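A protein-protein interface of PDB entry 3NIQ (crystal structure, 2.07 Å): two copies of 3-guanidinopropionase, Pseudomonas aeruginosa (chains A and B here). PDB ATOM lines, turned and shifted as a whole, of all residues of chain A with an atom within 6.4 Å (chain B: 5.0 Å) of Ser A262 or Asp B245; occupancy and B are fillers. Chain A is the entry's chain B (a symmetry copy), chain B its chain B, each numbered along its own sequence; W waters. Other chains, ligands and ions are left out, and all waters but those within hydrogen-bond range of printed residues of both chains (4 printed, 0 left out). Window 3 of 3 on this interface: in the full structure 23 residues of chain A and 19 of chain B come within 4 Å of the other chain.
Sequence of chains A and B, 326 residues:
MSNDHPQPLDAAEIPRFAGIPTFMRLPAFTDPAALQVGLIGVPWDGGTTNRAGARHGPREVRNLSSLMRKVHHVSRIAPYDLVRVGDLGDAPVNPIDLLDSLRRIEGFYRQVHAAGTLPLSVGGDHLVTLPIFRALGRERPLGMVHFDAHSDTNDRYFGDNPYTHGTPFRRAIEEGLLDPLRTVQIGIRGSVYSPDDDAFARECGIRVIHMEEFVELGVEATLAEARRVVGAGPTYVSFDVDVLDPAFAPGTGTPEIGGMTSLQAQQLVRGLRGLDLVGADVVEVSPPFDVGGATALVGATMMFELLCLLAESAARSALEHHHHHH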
ATOM      1  N   LEU A 244     -10.223  26.064  -5.795  1.00  0.00           N
ATOM      2  CA  LEU A 244     -10.923  24.826  -6.137  1.00  0.00           C
ATOM      3  C   LEU A 244     -10.125  23.622  -5.668  1.00  0.00           C
ATOM      4  O   LEU A 244      -8.884  23.648  -5.647  1.00  0.00           O
ATOM      5  CB  LEU A 244     -11.130  24.733  -7.658  1.00  0.00           C
ATOM      6  CG  LEU A 244     -12.003  25.800  -8.311  1.00  0.00           C
ATOM      7  CD1 LEU A 244     -11.823  25.749  -9.825  1.00  0.00           C
ATOM      8  CD2 LEU A 244     -13.484  25.611  -7.933  1.00  0.00           C
ATOM      9  N   ALA A 247      -9.180  18.254  -7.716  1.00  0.00           N
ATOM     10  CA  ALA A 247      -9.943  17.401  -8.632  1.00  0.00           C
ATOM     11  C   ALA A 247     -10.559  18.231  -9.764  1.00  0.00           C
ATOM     12  O   ALA A 247     -10.785  17.721 -10.852  1.00  0.00           O
ATOM     13  CB  ALA A 247     -11.002  16.624  -7.895  1.00  0.00           C
ATOM     14  N   PHE A 248     -10.822  19.511  -9.503  1.00  0.00           N
ATOM     15  CA  PHE A 248     -11.436  20.392 -10.494  1.00  0.00           C
ATOM     16  C   PHE A 248     -10.381  21.236 -11.152  1.00  0.00           C
ATOM     17  O   PHE A 248     -10.524  21.629 -12.307  1.00  0.00           O
ATOM     18  CB  PHE A 248     -12.495  21.295  -9.831  1.00  0.00           C
ATOM     19  CG  PHE A 248     -13.498  20.524  -9.016  1.00  0.00           C
ATOM     20  CD1 PHE A 248     -14.615  19.951  -9.623  1.00  0.00           C
ATOM     21  CD2 PHE A 248     -13.310  20.344  -7.658  1.00  0.00           C
ATOM     22  CE1 PHE A 248     -15.532  19.217  -8.871  1.00  0.00           C
ATOM     23  CE2 PHE A 248     -14.197  19.612  -6.908  1.00  0.00           C
ATOM     24  CZ  PHE A 248     -15.318  19.040  -7.520  1.00  0.00           C
ATOM     25  N   ALA A 249      -9.322  21.522 -10.404  1.00  0.00           N
ATOM     26  CA  ALA A 249      -8.264  22.378 -10.908  1.00  0.00           C
ATOM     27  C   ALA A 249      -6.898  21.811 -10.558  1.00  0.00           C
ATOM     28  O   ALA A 249      -6.200  22.352  -9.711  1.00  0.00           O
ATOM     29  CB  ALA A 249      -8.440  23.817 -10.371  1.00  0.00           C
ATOM     30  N   MET A 260     -13.019  23.968  -2.943  1.00  0.00           N
ATOM     31  CA  MET A 260     -14.322  24.343  -3.475  1.00  0.00           C
ATOM     32  C   MET A 260     -14.582  23.562  -4.766  1.00  0.00           C
ATOM     33  O   MET A 260     -13.649  23.267  -5.506  1.00  0.00           O
ATOM     34  CB  MET A 260     -14.282  25.853  -3.743  1.00  0.00           C
ATOM     35  CG  MET A 260     -15.555  26.522  -4.203  1.00  0.00           C
ATOM     36  SD  MET A 260     -15.317  28.326  -4.290  1.00  0.00           S
ATOM     37  CE  MET A 260     -14.889  28.763  -2.603  1.00  0.00           C
ATOM     38  N   THR A 261     -15.830  23.209  -5.031  1.00  0.00           N
ATOM     39  CA  THR A 261     -16.187  22.592  -6.317  1.00  0.00           C
ATOM     40  C   THR A 261     -16.347  23.688  -7.377  1.00  0.00           C
ATOM     41  O   THR A 261     -16.534  24.854  -7.037  1.00  0.00           O
ATOM     42  CB  THR A 261     -17.509  21.817  -6.216  1.00  0.00           C
ATOM     43  OG1 THR A 261     -18.583  22.744  -6.044  1.00  0.00           O
ATOM     44  CG2 THR A 261     -17.492  20.822  -5.027  1.00  0.00           C
ATOM     45  N   SER A 262     -16.283  23.318  -8.655  1.00  0.00           N
ATOM     46  CA  SER A 262     -16.518  24.263  -9.743  1.00  0.00           C
ATOM     47  C   SER A 262     -17.942  24.805  -9.642  1.00  0.00           C
ATOM     48  O   SER A 262     -18.187  25.987  -9.859  1.00  0.00           O
ATOM     49  CB  SER A 262     -16.324  23.589 -11.114  1.00  0.00           C
ATOM     50  OG  SER A 262     -14.958  23.335 -11.388  1.00  0.00           O
ATOM     51  N   LEU A 263     -18.884  23.927  -9.337  1.00  0.00           N
ATOM     52  CA  LEU A 263     -20.267  24.363  -9.147  1.00  0.00           C
ATOM     53  C   LEU A 263     -20.332  25.531  -8.149  1.00  0.00           C
ATOM     54  O   LEU A 263     -20.914  26.583  -8.451  1.00  0.00           O
ATOM     55  CB  LEU A 263     -21.143  23.192  -8.697  1.00  0.00           C
ATOM     56  CG  LEU A 263     -22.617  23.457  -8.351  1.00  0.00           C
ATOM     57  CD1 LEU A 263     -23.380  24.138  -9.491  1.00  0.00           C
ATOM     58  CD2 LEU A 263     -23.281  22.159  -7.955  1.00  0.00           C
ATOM     59  N   GLN A 264     -19.700  25.354  -6.991  1.00  0.00           N
ATOM     60  CA  GLN A 264     -19.699  26.376  -5.934  1.00  0.00           C
ATOM     61  C   GLN A 264     -19.070  27.682  -6.407  1.00  0.00           C
ATOM     62  O   GLN A 264     -19.600  28.769  -6.154  1.00  0.00           O
ATOM     63  CB  GLN A 264     -19.019  25.859  -4.662  1.00  0.00           C
ATOM     64  CG  GLN A 264     -19.827  24.783  -3.920  1.00  0.00           C
ATOM     65  CD  GLN A 264     -19.029  24.059  -2.843  1.00  0.00           C
ATOM     66  OE1 GLN A 264     -17.811  23.866  -2.957  1.00  0.00           O
ATOM     67  NE2 GLN A 264     -19.721  23.645  -1.783  1.00  0.00           N
ATOM     68  N   ALA A 265     -17.962  27.575  -7.130  1.00  0.00           N
ATOM     69  CA  ALA A 265     -17.297  28.748  -7.655  1.00  0.00           C
ATOM     70  C   ALA A 265     -18.264  29.516  -8.555  1.00  0.00           C
ATOM     71  O   ALA A 265     -18.360  30.730  -8.453  1.00  0.00           O
ATOM     72  CB  ALA A 265     -16.020  28.367  -8.403  1.00  0.00           C
ATOM     73  N   GLN A 266     -19.011  28.806  -9.397  1.00  0.00           N
ATOM     74  CA  GLN A 266     -19.979  29.449 -10.285  1.00  0.00           C
ATOM     75  C   GLN A 266     -21.155  30.093  -9.545  1.00  0.00           C
ATOM     76  O   GLN A 266     -21.585  31.180  -9.906  1.00  0.00           O
ATOM     77  CB  GLN A 266     -20.511  28.466 -11.318  1.00  0.00           C
ATOM     78  CG  GLN A 266     -19.530  28.111 -12.417  1.00  0.00           C
ATOM     79  CD  GLN A 266     -20.101  27.067 -13.352  1.00  0.00           C
ATOM     80  OE1 GLN A 266     -20.475  25.985 -12.920  1.00  0.00           O
ATOM     81  NE2 GLN A 266     -20.174  27.385 -14.635  1.00  0.00           N
ATOM     82  N   GLN A 267     -21.672  29.434  -8.516  1.00  0.00           N
ATOM     83  CA  GLN A 267     -22.763  30.015  -7.727  1.00  0.00           C
ATOM     84  C   GLN A 267     -22.261  31.294  -7.045  1.00  0.00           C
ATOM     85  O   GLN A 267     -22.913  32.328  -7.109  1.00  0.00           O
ATOM     86  CB  GLN A 267     -23.266  29.038  -6.670  1.00  0.00           C
ATOM     87  CG  GLN A 267     -23.894  27.759  -7.198  1.00  0.00           C
ATOM     88  CD  GLN A 267     -23.858  26.663  -6.148  1.00  0.00           C
ATOM     89  OE1 GLN A 267     -22.929  26.601  -5.338  1.00  0.00           O
ATOM     90  NE2 GLN A 267     -24.864  25.795  -6.152  1.00  0.00           N
ATOM     91  N   VAL A 298     -11.717  25.289 -16.837  1.00  0.00           N
ATOM     92  CA  VAL A 298     -12.193  25.962 -15.634  1.00  0.00           C
ATOM     93  C   VAL A 298     -11.887  27.467 -15.757  1.00  0.00           C
ATOM     94  O   VAL A 298     -12.771  28.301 -15.557  1.00  0.00           O
ATOM     95  CB  VAL A 298     -11.574  25.365 -14.338  1.00  0.00           C
ATOM     96  CG1 VAL A 298     -11.821  26.304 -13.130  1.00  0.00           C
ATOM     97  CG2 VAL A 298     -12.123  23.975 -14.061  1.00  0.00           C
ATOM     98  N   MET A 302     -14.706  30.351 -15.818  1.00  0.00           N
ATOM     99  CA  MET A 302     -14.792  31.385 -14.774  1.00  0.00           C
ATOM    100  C   MET A 302     -14.620  32.764 -15.401  1.00  0.00           C
ATOM    101  O   MET A 302     -15.295  33.721 -14.993  1.00  0.00           O
ATOM    102  CB  MET A 302     -13.783  31.157 -13.654  1.00  0.00           C
ATOM    103  CG  MET A 302     -14.049  29.901 -12.824  1.00  0.00           C
ATOM    104  SD  MET A 302     -15.778  29.621 -12.364  1.00  0.00           S
ATOM    105  CE  MET A 302     -16.135  31.062 -11.349  1.00  0.00           C
ATOM    106  N   ARG B 189     -26.904  22.610 -18.376  1.00  0.00           N
ATOM    107  CA  ARG B 189     -26.110  23.759 -17.908  1.00  0.00           C
ATOM    108  C   ARG B 189     -25.143  24.280 -18.968  1.00  0.00           C
ATOM    109  O   ARG B 189     -24.949  23.665 -20.017  1.00  0.00           O
ATOM    110  CB  ARG B 189     -25.299  23.382 -16.658  1.00  0.00           C
ATOM    111  CG  ARG B 189     -24.232  22.327 -16.938  1.00  0.00           C
ATOM    112  CD  ARG B 189     -23.402  22.014 -15.705  1.00  0.00           C
ATOM    113  NE  ARG B 189     -22.389  20.998 -16.005  1.00  0.00           N
ATOM    114  CZ  ARG B 189     -22.625  19.685 -16.030  1.00  0.00           C
ATOM    115  NH1 ARG B 189     -23.844  19.209 -15.782  1.00  0.00           N
ATOM    116  NH2 ARG B 189     -21.637  18.840 -16.299  1.00  0.00           N
ATOM    117  N   VAL B 243     -23.093  14.897 -18.187  1.00  0.00           N
ATOM    118  CA  VAL B 243     -23.948  15.399 -17.113  1.00  0.00           C
ATOM    119  C   VAL B 243     -23.090  15.553 -15.858  1.00  0.00           C
ATOM    120  O   VAL B 243     -23.305  16.452 -15.042  1.00  0.00           O
ATOM    121  CB  VAL B 243     -25.190  14.483 -16.852  1.00  0.00           C
ATOM    122  CG1 VAL B 243     -24.794  13.143 -16.200  1.00  0.00           C
ATOM    123  CG2 VAL B 243     -26.258  15.218 -15.975  1.00  0.00           C
ATOM    124  N   LEU B 244     -22.094  14.683 -15.732  1.00  0.00           N
ATOM    125  CA  LEU B 244     -21.166  14.710 -14.602  1.00  0.00           C
ATOM    126  C   LEU B 244     -20.166  15.842 -14.766  1.00  0.00           C
ATOM    127  O   LEU B 244     -19.783  16.195 -15.892  1.00  0.00           O
ATOM    128  CB  LEU B 244     -20.407  13.376 -14.503  1.00  0.00           C
ATOM    129  CG  LEU B 244     -21.230  12.122 -14.228  1.00  0.00           C
ATOM    130  CD1 LEU B 244     -20.378  10.885 -14.494  1.00  0.00           C
ATOM    131  CD2 LEU B 244     -21.761  12.114 -12.783  1.00  0.00           C
ATOM    132  N   ASP B 245     -19.723  16.402 -13.641  1.00  0.00           N
ATOM    133  CA  ASP B 245     -18.611  17.333 -13.685  1.00  0.00           C
ATOM    134  C   ASP B 245     -17.406  16.660 -14.339  1.00  0.00           C
ATOM    135  O   ASP B 245     -17.208  15.449 -14.177  1.00  0.00           O
ATOM    136  CB  ASP B 245     -18.270  17.839 -12.284  1.00  0.00           C
ATOM    137  CG  ASP B 245     -17.346  19.040 -12.316  1.00  0.00           C
ATOM    138  OD1 ASP B 245     -17.854  20.183 -12.286  1.00  0.00           O
ATOM    139  OD2 ASP B 245     -16.116  18.837 -12.407  1.00  0.00           O
ATOM    140  N   PRO B 246     -16.625  17.435 -15.117  1.00  0.00           N
ATOM    141  CA  PRO B 246     -15.383  16.966 -15.760  1.00  0.00           C
ATOM    142  C   PRO B 246     -14.412  16.292 -14.785  1.00  0.00           C
ATOM    143  O   PRO B 246     -13.572  15.508 -15.202  1.00  0.00           O
ATOM    144  CB  PRO B 246     -14.768  18.248 -16.300  1.00  0.00           C
ATOM    145  CG  PRO B 246     -15.967  19.123 -16.602  1.00  0.00           C
ATOM    146  CD  PRO B 246     -17.013  18.784 -15.586  1.00  0.00           C
ATOM    147  N   ALA B 247     -14.533  16.581 -13.492  1.00  0.00           N
ATOM    148  CA  ALA B 247     -13.651  15.932 -12.517  1.00  0.00           C
ATOM    149  C   ALA B 247     -13.961  14.435 -12.412  1.00  0.00           C
ATOM    150  O   ALA B 247     -13.088  13.645 -12.082  1.00  0.00           O
ATOM    151  CB  ALA B 247     -13.748  16.599 -11.170  1.00  0.00           C
ATOM    152  N   PHE B 248     -15.204  14.052 -12.701  1.00  0.00           N
ATOM    153  CA  PHE B 248     -15.624  12.656 -12.608  1.00  0.00           C
ATOM    154  C   PHE B 248     -15.621  12.028 -13.974  1.00  0.00           C
ATOM    155  O   PHE B 248     -15.411  10.825 -14.109  1.00  0.00           O
ATOM    156  CB  PHE B 248     -17.031  12.555 -11.986  1.00  0.00           C
ATOM    157  CG  PHE B 248     -17.153  13.303 -10.684  1.00  0.00           C
ATOM    158  CD1 PHE B 248     -16.767  12.705  -9.486  1.00  0.00           C
ATOM    159  CD2 PHE B 248     -17.619  14.604 -10.663  1.00  0.00           C
ATOM    160  CE1 PHE B 248     -16.858  13.407  -8.283  1.00  0.00           C
ATOM    161  CE2 PHE B 248     -17.701  15.311  -9.489  1.00  0.00           C
ATOM    162  CZ  PHE B 248     -17.314  14.708  -8.287  1.00  0.00           C
ATOM    163  N   ALA B 249     -15.866  12.851 -14.987  1.00  0.00           N
ATOM    164  CA  ALA B 249     -15.948  12.352 -16.347  1.00  0.00           C
ATOM    165  C   ALA B 249     -15.210  13.273 -17.305  1.00  0.00           C
ATOM    166  O   ALA B 249     -15.830  13.973 -18.093  1.00  0.00           O
ATOM    167  CB  ALA B 249     -17.427  12.165 -16.759  1.00  0.00           C
ATOM    168  N   GLU B 256     -18.853  20.550 -19.626  1.00  0.00           N
ATOM    169  CA  GLU B 256     -19.321  21.820 -19.054  1.00  0.00           C
ATOM    170  C   GLU B 256     -19.049  21.690 -17.565  1.00  0.00           C
ATOM    171  O   GLU B 256     -19.466  20.720 -16.948  1.00  0.00           O
ATOM    172  CB  GLU B 256     -20.833  22.048 -19.275  1.00  0.00           C
ATOM    173  CG  GLU B 256     -21.367  21.809 -20.699  1.00  0.00           C
ATOM    174  CD  GLU B 256     -21.075  22.961 -21.687  1.00  0.00           C
ATOM    175  OE1 GLU B 256     -20.590  24.022 -21.260  1.00  0.00           O
ATOM    176  OE2 GLU B 256     -21.337  22.804 -22.903  1.00  0.00           O
ATOM    177  N   ILE B 257     -18.352  22.653 -16.974  1.00  0.00           N
ATOM    178  CA  ILE B 257     -18.018  22.540 -15.555  1.00  0.00           C
ATOM    179  C   ILE B 257     -19.251  22.736 -14.672  1.00  0.00           C
ATOM    180  O   ILE B 257     -20.335  23.111 -15.154  1.00  0.00           O
ATOM    181  CB  ILE B 257     -16.906  23.534 -15.152  1.00  0.00           C
ATOM    182  CG1 ILE B 257     -17.404  24.985 -15.277  1.00  0.00           C
ATOM    183  CG2 ILE B 257     -15.668  23.325 -16.060  1.00  0.00           C
ATOM    184  CD1 ILE B 257     -16.607  25.972 -14.428  1.00  0.00           C
ATOM    185  N   GLY B 258     -19.075  22.483 -13.380  1.00  0.00           N
ATOM    186  CA  GLY B 258     -20.144  22.656 -12.411  1.00  0.00           C
ATOM    187  C   GLY B 258     -21.231  21.609 -12.527  1.00  0.00           C
ATOM    188  O   GLY B 258     -22.426  21.927 -12.461  1.00  0.00           O
ATOM    189  N   GLY B 259     -20.816  20.350 -12.656  1.00  0.00           N
ATOM    190  CA  GLY B 259     -21.749  19.258 -12.907  1.00  0.00           C
ATOM    191  C   GLY B 259     -22.061  18.324 -11.754  1.00  0.00           C
ATOM    192  O   GLY B 259     -21.700  18.578 -10.609  1.00  0.00           O
ATOM    193  N   MET B 260     -22.764  17.245 -12.081  1.00  0.00           N
ATOM    194  CA  MET B 260     -23.237  16.264 -11.113  1.00  0.00           C
ATOM    195  C   MET B 260     -22.057  15.402 -10.654  1.00  0.00           C
ATOM    196  O   MET B 260     -21.142  15.146 -11.429  1.00  0.00           O
ATOM    197  CB  MET B 260     -24.300  15.412 -11.817  1.00  0.00           C
ATOM    198  CG  MET B 260     -25.034  14.380 -10.996  1.00  0.00           C
ATOM    199  SD  MET B 260     -26.357  13.616 -11.989  1.00  0.00           S
ATOM    200  CE  MET B 260     -27.400  15.011 -12.420  1.00  0.00           C
HETATM  201  O   HOH W   1     -11.399  18.037 -13.600  1.00  0.00           O
HETATM  202  O   HOH W   2     -15.083  21.214 -13.164  1.00  0.00           O
HETATM  203  O   HOH W   3     -18.401  21.191  -9.535  1.00  0.00           O
HETATM  204  O   HOH W   4     -21.049  25.439 -16.668  1.00  0.00           O
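Of the 14 printed residues of chain A, 5 touch a printed residue of chain B. Hydrophobic or aromatic side chains of chain A that line the printed part of chain B: Phe A248 and Leu A263. Hydrophobic or aromatic side chains of chain B that line the printed part of chain A: Ala B247 and Ile B257.
Among the printed residues, merely in contact across the chains: Ala A247 with Ala B247 (3.2 Å), Phe A248 with Asp B245 (3.4 Å), Gln A266 with Gly B258 (3.4 Å), Leu A263 with Gly B258 (3.6 Å), Gln A266 with Ile B257 (3.6 Å), Ser A262 with Gly B258 (3.7 Å), Phe A248 with Ala B247 (3.8 Å) and Ser A262 with Asp B245 (3.9 Å).
NE of Arg B189 is in hydrogen-bond range of O of Ile B257, at 3.1 Å. N of Ala B247 lies within hydrogen-bond range of OD2 of Asp B245. The side-chain carboxylate of Asp B245 sits at hydrogen-bond distance from the backbone NH of Gly B258 (2.8 Å). The side-chain carboxylate (OD1) of Asp B245 lies within hydrogen-bond range of the backbone NH (N) of Gly B259 (3.0 Å). The backbone NH of Asp B245 is in hydrogen-bond range of the backbone carbonyl oxygen of Met B260 (2.9 Å).
Of the printed residues of chain B, Ala A247 touches Ala B247 (3.2 Å). Of chain B, only Asp B245 and Gly B258 come within 4 Å of Ser A262. Printed residues of chain B within 4 Å of Leu A263: Gly B258 (3.6 Å). Asp B245 touches just these residues of chain A: Phe A248 and Ser A262. The nearest residue of chain A that does not touch Asp B245 is Leu A263 (4.9 Å).
Ala B247 touches its own counterpart, Ala A247. Phe A248 touches Ala B247, but with the chains exchanged Ala A247 does not touch Phe B248 (6.0 Å). Positions printed for both chains: 244, 247, 248, 249 and 260.
Water W2 lies within hydrogen-bond range of OD2 of Asp B245 and OG of Ser A262. Water W3 lies within hydrogen-bond range of the backbone NH (N) of Leu A263, the side-chain carboxylate (OD1) of Asp B245 and the backbone NH (N) of Ser A262. Water W1 lies within hydrogen-bond range of O of Ala A247 and N of Ala B247. Water W4 lies within hydrogen-bond range of the backbone carbonyl oxygen (O) of Ile B257 (2.9 Å) and the side-chain amide nitrogen (NE2) of Gln A266 (2.9 Å).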
